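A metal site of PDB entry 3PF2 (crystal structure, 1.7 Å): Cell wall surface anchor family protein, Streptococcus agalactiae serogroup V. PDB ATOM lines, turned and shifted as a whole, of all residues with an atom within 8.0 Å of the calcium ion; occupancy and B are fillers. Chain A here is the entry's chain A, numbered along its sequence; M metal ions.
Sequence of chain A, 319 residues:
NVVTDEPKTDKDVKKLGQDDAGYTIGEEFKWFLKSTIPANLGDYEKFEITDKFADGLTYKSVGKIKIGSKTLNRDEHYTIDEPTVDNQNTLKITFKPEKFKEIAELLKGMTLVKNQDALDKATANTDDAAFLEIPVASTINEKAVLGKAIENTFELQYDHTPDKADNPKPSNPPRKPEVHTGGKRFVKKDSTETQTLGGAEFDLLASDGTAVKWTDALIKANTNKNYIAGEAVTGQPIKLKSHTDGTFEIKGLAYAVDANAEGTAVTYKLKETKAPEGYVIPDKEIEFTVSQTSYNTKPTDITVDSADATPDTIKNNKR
O of Lys 46 lies within hydrogen-bond range of N of Asp 159 (3.0 Å). The side-chain carboxylate (OE2) of Glu 45 is in hydrogen-bond range of the backbone NH (N) of Lys 164, at 2.8 Å.
The calcium ion is bound by the side-chain carboxylate (OD1) of Asp 159 (2.4 Å), the side-chain carboxylate (OD1) of Asp 163 (2.4 Å), the side-chain amide oxygen (OD1) of Asn 167 (2.4 Å), the side-chain carboxylate (OE1) of Glu 45 (2.4 Å), the backbone carbonyl oxygen (O) of Ala 165 (2.5 Å), the backbone carbonyl oxygen (O) of Thr 161 (2.5 Å), the side-chain carboxylate (OD2) of Asp 159 (2.6 Å) and the side-chain hydroxyl (OG1) of Thr 161 (2.6 Å). The calcium ion has eight donor atoms within binding distance.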
ATOM      1  N   ASP A  43      -6.359  -2.375  -6.578  1.00  0.00           N
ATOM      2  CA  ASP A  43      -6.926  -3.009  -5.386  1.00  0.00           C
ATOM      3  C   ASP A  43      -8.112  -2.257  -4.781  1.00  0.00           C
ATOM      4  O   ASP A  43      -8.869  -2.813  -3.982  1.00  0.00           O
ATOM      5  CB  ASP A  43      -5.868  -3.117  -4.292  1.00  0.00           C
ATOM      6  CG  ASP A  43      -4.780  -4.120  -4.611  1.00  0.00           C
ATOM      7  OD1 ASP A  43      -4.951  -4.974  -5.510  1.00  0.00           O
ATOM      8  OD2 ASP A  43      -3.735  -4.043  -3.923  1.00  0.00           O
ATOM      9  N   TYR A  44      -8.274  -0.984  -5.138  1.00  0.00           N
ATOM     10  CA  TYR A  44      -9.205  -0.113  -4.415  1.00  0.00           C
ATOM     11  C   TYR A  44     -10.663  -0.512  -4.632  1.00  0.00           C
ATOM     12  O   TYR A  44     -11.057  -0.905  -5.742  1.00  0.00           O
ATOM     13  CB  TYR A  44      -8.970   1.361  -4.789  1.00  0.00           C
ATOM     14  CG  TYR A  44      -7.813   2.023  -4.027  1.00  0.00           C
ATOM     15  CD1 TYR A  44      -6.552   1.428  -3.965  1.00  0.00           C
ATOM     16  CD2 TYR A  44      -7.997   3.263  -3.392  1.00  0.00           C
ATOM     17  CE1 TYR A  44      -5.488   2.036  -3.274  1.00  0.00           C
ATOM     18  CE2 TYR A  44      -6.955   3.878  -2.705  1.00  0.00           C
ATOM     19  CZ  TYR A  44      -5.711   3.271  -2.639  1.00  0.00           C
ATOM     20  OH  TYR A  44      -4.698   3.873  -1.948  1.00  0.00           O
ATOM     21  N   GLU A  45     -11.458  -0.425  -3.555  1.00  0.00           N
ATOM     22  CA  GLU A  45     -12.884  -0.778  -3.573  1.00  0.00           C
ATOM     23  C   GLU A  45     -13.808   0.442  -3.564  1.00  0.00           C
ATOM     24  O   GLU A  45     -15.039   0.304  -3.704  1.00  0.00           O
ATOM     25  CB  GLU A  45     -13.207  -1.717  -2.398  1.00  0.00           C
ATOM     26  CG  GLU A  45     -12.264  -2.930  -2.321  1.00  0.00           C
ATOM     27  CD  GLU A  45     -12.625  -3.881  -1.187  1.00  0.00           C
ATOM     28  OE1 GLU A  45     -13.099  -3.413  -0.143  1.00  0.00           O
ATOM     29  OE2 GLU A  45     -12.404  -5.120  -1.352  1.00  0.00           O
ATOM     30  N   LYS A  46     -13.225   1.638  -3.394  1.00  0.00           N
ATOM     31  CA  LYS A  46     -13.961   2.892  -3.443  1.00  0.00           C
ATOM     32  C   LYS A  46     -12.985   4.029  -3.756  1.00  0.00           C
ATOM     33  O   LYS A  46     -11.847   4.032  -3.292  1.00  0.00           O
ATOM     34  CB  LYS A  46     -14.646   3.187  -2.099  1.00  0.00           C
ATOM     35  CG  LYS A  46     -15.686   4.305  -2.163  1.00  0.00           C
ATOM     36  CD  LYS A  46     -16.152   4.773  -0.792  1.00  0.00           C
ATOM     37  CE  LYS A  46     -16.919   3.703  -0.036  1.00  0.00           C
ATOM     38  NZ  LYS A  46     -18.077   3.131  -0.792  1.00  0.00           N
ATOM     39  N   TYR A 158     -11.681   6.954   0.090  1.00  0.00           N
ATOM     40  CA  TYR A 158     -11.025   5.880  -0.662  1.00  0.00           C
ATOM     41  C   TYR A 158     -10.967   4.605   0.179  1.00  0.00           C
ATOM     42  O   TYR A 158     -10.831   4.663   1.405  1.00  0.00           O
ATOM     43  CB  TYR A 158      -9.617   6.305  -1.080  1.00  0.00           C
ATOM     44  CG  TYR A 158      -8.650   6.484   0.071  1.00  0.00           C
ATOM     45  CD1 TYR A 158      -7.879   5.406   0.537  1.00  0.00           C
ATOM     46  CD2 TYR A 158      -8.511   7.733   0.702  1.00  0.00           C
ATOM     47  CE1 TYR A 158      -6.988   5.558   1.597  1.00  0.00           C
ATOM     48  CE2 TYR A 158      -7.611   7.891   1.771  1.00  0.00           C
ATOM     49  CZ  TYR A 158      -6.859   6.803   2.196  1.00  0.00           C
ATOM     50  OH  TYR A 158      -5.988   6.959   3.220  1.00  0.00           O
ATOM     51  N   ASP A 159     -11.099   3.459  -0.495  1.00  0.00           N
ATOM     52  CA  ASP A 159     -10.977   2.168   0.161  1.00  0.00           C
ATOM     53  C   ASP A 159      -9.832   1.429  -0.528  1.00  0.00           C
ATOM     54  O   ASP A 159      -9.988   0.916  -1.659  1.00  0.00           O
ATOM     55  CB  ASP A 159     -12.302   1.376   0.087  1.00  0.00           C
ATOM     56  CG  ASP A 159     -12.256   0.046   0.854  1.00  0.00           C
ATOM     57  OD1 ASP A 159     -11.154  -0.493   1.045  1.00  0.00           O
ATOM     58  OD2 ASP A 159     -13.331  -0.449   1.235  1.00  0.00           O
ATOM     59  N   HIS A 160      -8.683   1.407   0.154  1.00  0.00           N
ATOM     60  CA  HIS A 160      -7.431   0.839  -0.351  1.00  0.00           C
ATOM     61  C   HIS A 160      -7.260  -0.647  -0.055  1.00  0.00           C
ATOM     62  O   HIS A 160      -6.267  -1.250  -0.485  1.00  0.00           O
ATOM     63  CB  HIS A 160      -6.211   1.631   0.185  1.00  0.00           C
ATOM     64  CG  HIS A 160      -5.785   1.262   1.579  1.00  0.00           C
ATOM     65  ND1 HIS A 160      -4.732   0.415   1.833  1.00  0.00           N
ATOM     66  CD2 HIS A 160      -6.223   1.684   2.786  1.00  0.00           C
ATOM     67  CE1 HIS A 160      -4.561   0.291   3.138  1.00  0.00           C
ATOM     68  NE2 HIS A 160      -5.466   1.046   3.738  1.00  0.00           N
ATOM     69  N   THR A 161      -8.197  -1.212   0.703  1.00  0.00           N
ATOM     70  CA  THR A 161      -8.078  -2.620   1.116  1.00  0.00           C
ATOM     71  C   THR A 161      -8.942  -3.569   0.288  1.00  0.00           C
ATOM     72  O   THR A 161     -10.156  -3.475   0.323  1.00  0.00           O
ATOM     73  CB  THR A 161      -8.374  -2.810   2.615  1.00  0.00           C
ATOM     74  OG1 THR A 161      -9.646  -2.225   2.937  1.00  0.00           O
ATOM     75  CG2 THR A 161      -7.277  -2.156   3.452  1.00  0.00           C
ATOM     76  N   PRO A 162      -8.314  -4.512  -0.456  1.00  0.00           N
ATOM     77  CA  PRO A 162      -9.075  -5.484  -1.245  1.00  0.00           C
ATOM     78  C   PRO A 162      -9.592  -6.614  -0.349  1.00  0.00           C
ATOM     79  O   PRO A 162      -9.328  -7.793  -0.614  1.00  0.00           O
ATOM     80  CB  PRO A 162      -8.040  -5.994  -2.257  1.00  0.00           C
ATOM     81  CG  PRO A 162      -6.718  -5.876  -1.558  1.00  0.00           C
ATOM     82  CD  PRO A 162      -6.863  -4.714  -0.560  1.00  0.00           C
ATOM     83  N   ASP A 163     -10.333  -6.260   0.693  1.00  0.00           N
ATOM     84  CA  ASP A 163     -10.773  -7.223   1.696  1.00  0.00           C
ATOM     85  C   ASP A 163     -12.268  -7.577   1.621  1.00  0.00           C
ATOM     86  O   ASP A 163     -12.807  -8.253   2.506  1.00  0.00           O
ATOM     87  CB  ASP A 163     -10.372  -6.742   3.107  1.00  0.00           C
ATOM     88  CG  ASP A 163     -11.011  -5.409   3.489  1.00  0.00           C
ATOM     89  OD1 ASP A 163     -11.677  -4.783   2.634  1.00  0.00           O
ATOM     90  OD2 ASP A 163     -10.862  -5.003   4.654  1.00  0.00           O
ATOM     91  N   LYS A 164     -12.940  -7.120   0.555  1.00  0.00           N
ATOM     92  CA  LYS A 164     -14.382  -7.339   0.370  1.00  0.00           C
ATOM     93  C   LYS A 164     -15.219  -6.731   1.495  1.00  0.00           C
ATOM     94  O   LYS A 164     -16.356  -7.137   1.747  1.00  0.00           O
ATOM     95  CB  LYS A 164     -14.691  -8.838   0.228  1.00  0.00           C
ATOM     96  CG  LYS A 164     -13.862  -9.542  -0.813  1.00  0.00           C
ATOM     97  CD  LYS A 164     -14.174 -11.028  -0.798  1.00  0.00           C
ATOM     98  CE  LYS A 164     -13.033 -11.814  -1.392  1.00  0.00           C
ATOM     99  NZ  LYS A 164     -13.410 -13.260  -1.518  1.00  0.00           N
ATOM    100  N   ALA A 165     -14.643  -5.731   2.151  1.00  0.00           N
ATOM    101  CA  ALA A 165     -15.336  -5.065   3.238  1.00  0.00           C
ATOM    102  C   ALA A 165     -15.307  -3.569   2.983  1.00  0.00           C
ATOM    103  O   ALA A 165     -14.279  -3.026   2.600  1.00  0.00           O
ATOM    104  CB  ALA A 165     -14.663  -5.393   4.576  1.00  0.00           C
ATOM    105  N   ASP A 166     -16.454  -2.939   3.218  1.00  0.00           N
ATOM    106  CA  ASP A 166     -16.657  -1.519   2.959  1.00  0.00           C
ATOM    107  C   ASP A 166     -16.069  -0.700   4.128  1.00  0.00           C
ATOM    108  O   ASP A 166     -16.748  -0.507   5.135  1.00  0.00           O
ATOM    109  CB  ASP A 166     -18.156  -1.255   2.815  1.00  0.00           C
ATOM    110  CG  ASP A 166     -18.482   0.192   2.428  1.00  0.00           C
ATOM    111  OD1 ASP A 166     -17.632   0.867   1.824  1.00  0.00           O
ATOM    112  OD2 ASP A 166     -19.613   0.627   2.714  1.00  0.00           O
ATOM    113  N   ASN A 167     -14.831  -0.228   3.974  1.00  0.00           N
ATOM    114  CA  ASN A 167     -14.104   0.466   5.042  1.00  0.00           C
ATOM    115  C   ASN A 167     -13.252   1.634   4.534  1.00  0.00           C
ATOM    116  O   ASN A 167     -12.019   1.620   4.652  1.00  0.00           O
ATOM    117  CB  ASN A 167     -13.297  -0.529   5.889  1.00  0.00           C
ATOM    118  CG  ASN A 167     -12.602  -1.593   5.048  1.00  0.00           C
ATOM    119  OD1 ASN A 167     -12.213  -1.361   3.896  1.00  0.00           O
ATOM    120  ND2 ASN A 167     -12.441  -2.793   5.624  1.00  0.00           N
ATOM    121  N   PRO A 168     -13.912   2.652   3.970  1.00  0.00           N
ATOM    122  CA  PRO A 168     -13.153   3.765   3.392  1.00  0.00           C
ATOM    123  C   PRO A 168     -12.530   4.704   4.447  1.00  0.00           C
ATOM    124  O   PRO A 168     -12.906   4.666   5.637  1.00  0.00           O
ATOM    125  CB  PRO A 168     -14.220   4.519   2.599  1.00  0.00           C
ATOM    126  CG  PRO A 168     -15.481   4.262   3.357  1.00  0.00           C
ATOM    127  CD  PRO A 168     -15.358   2.826   3.781  1.00  0.00           C
HETATM  128 CA    CA M   1     -11.976  -2.562   1.820  1.00  0.00          CA
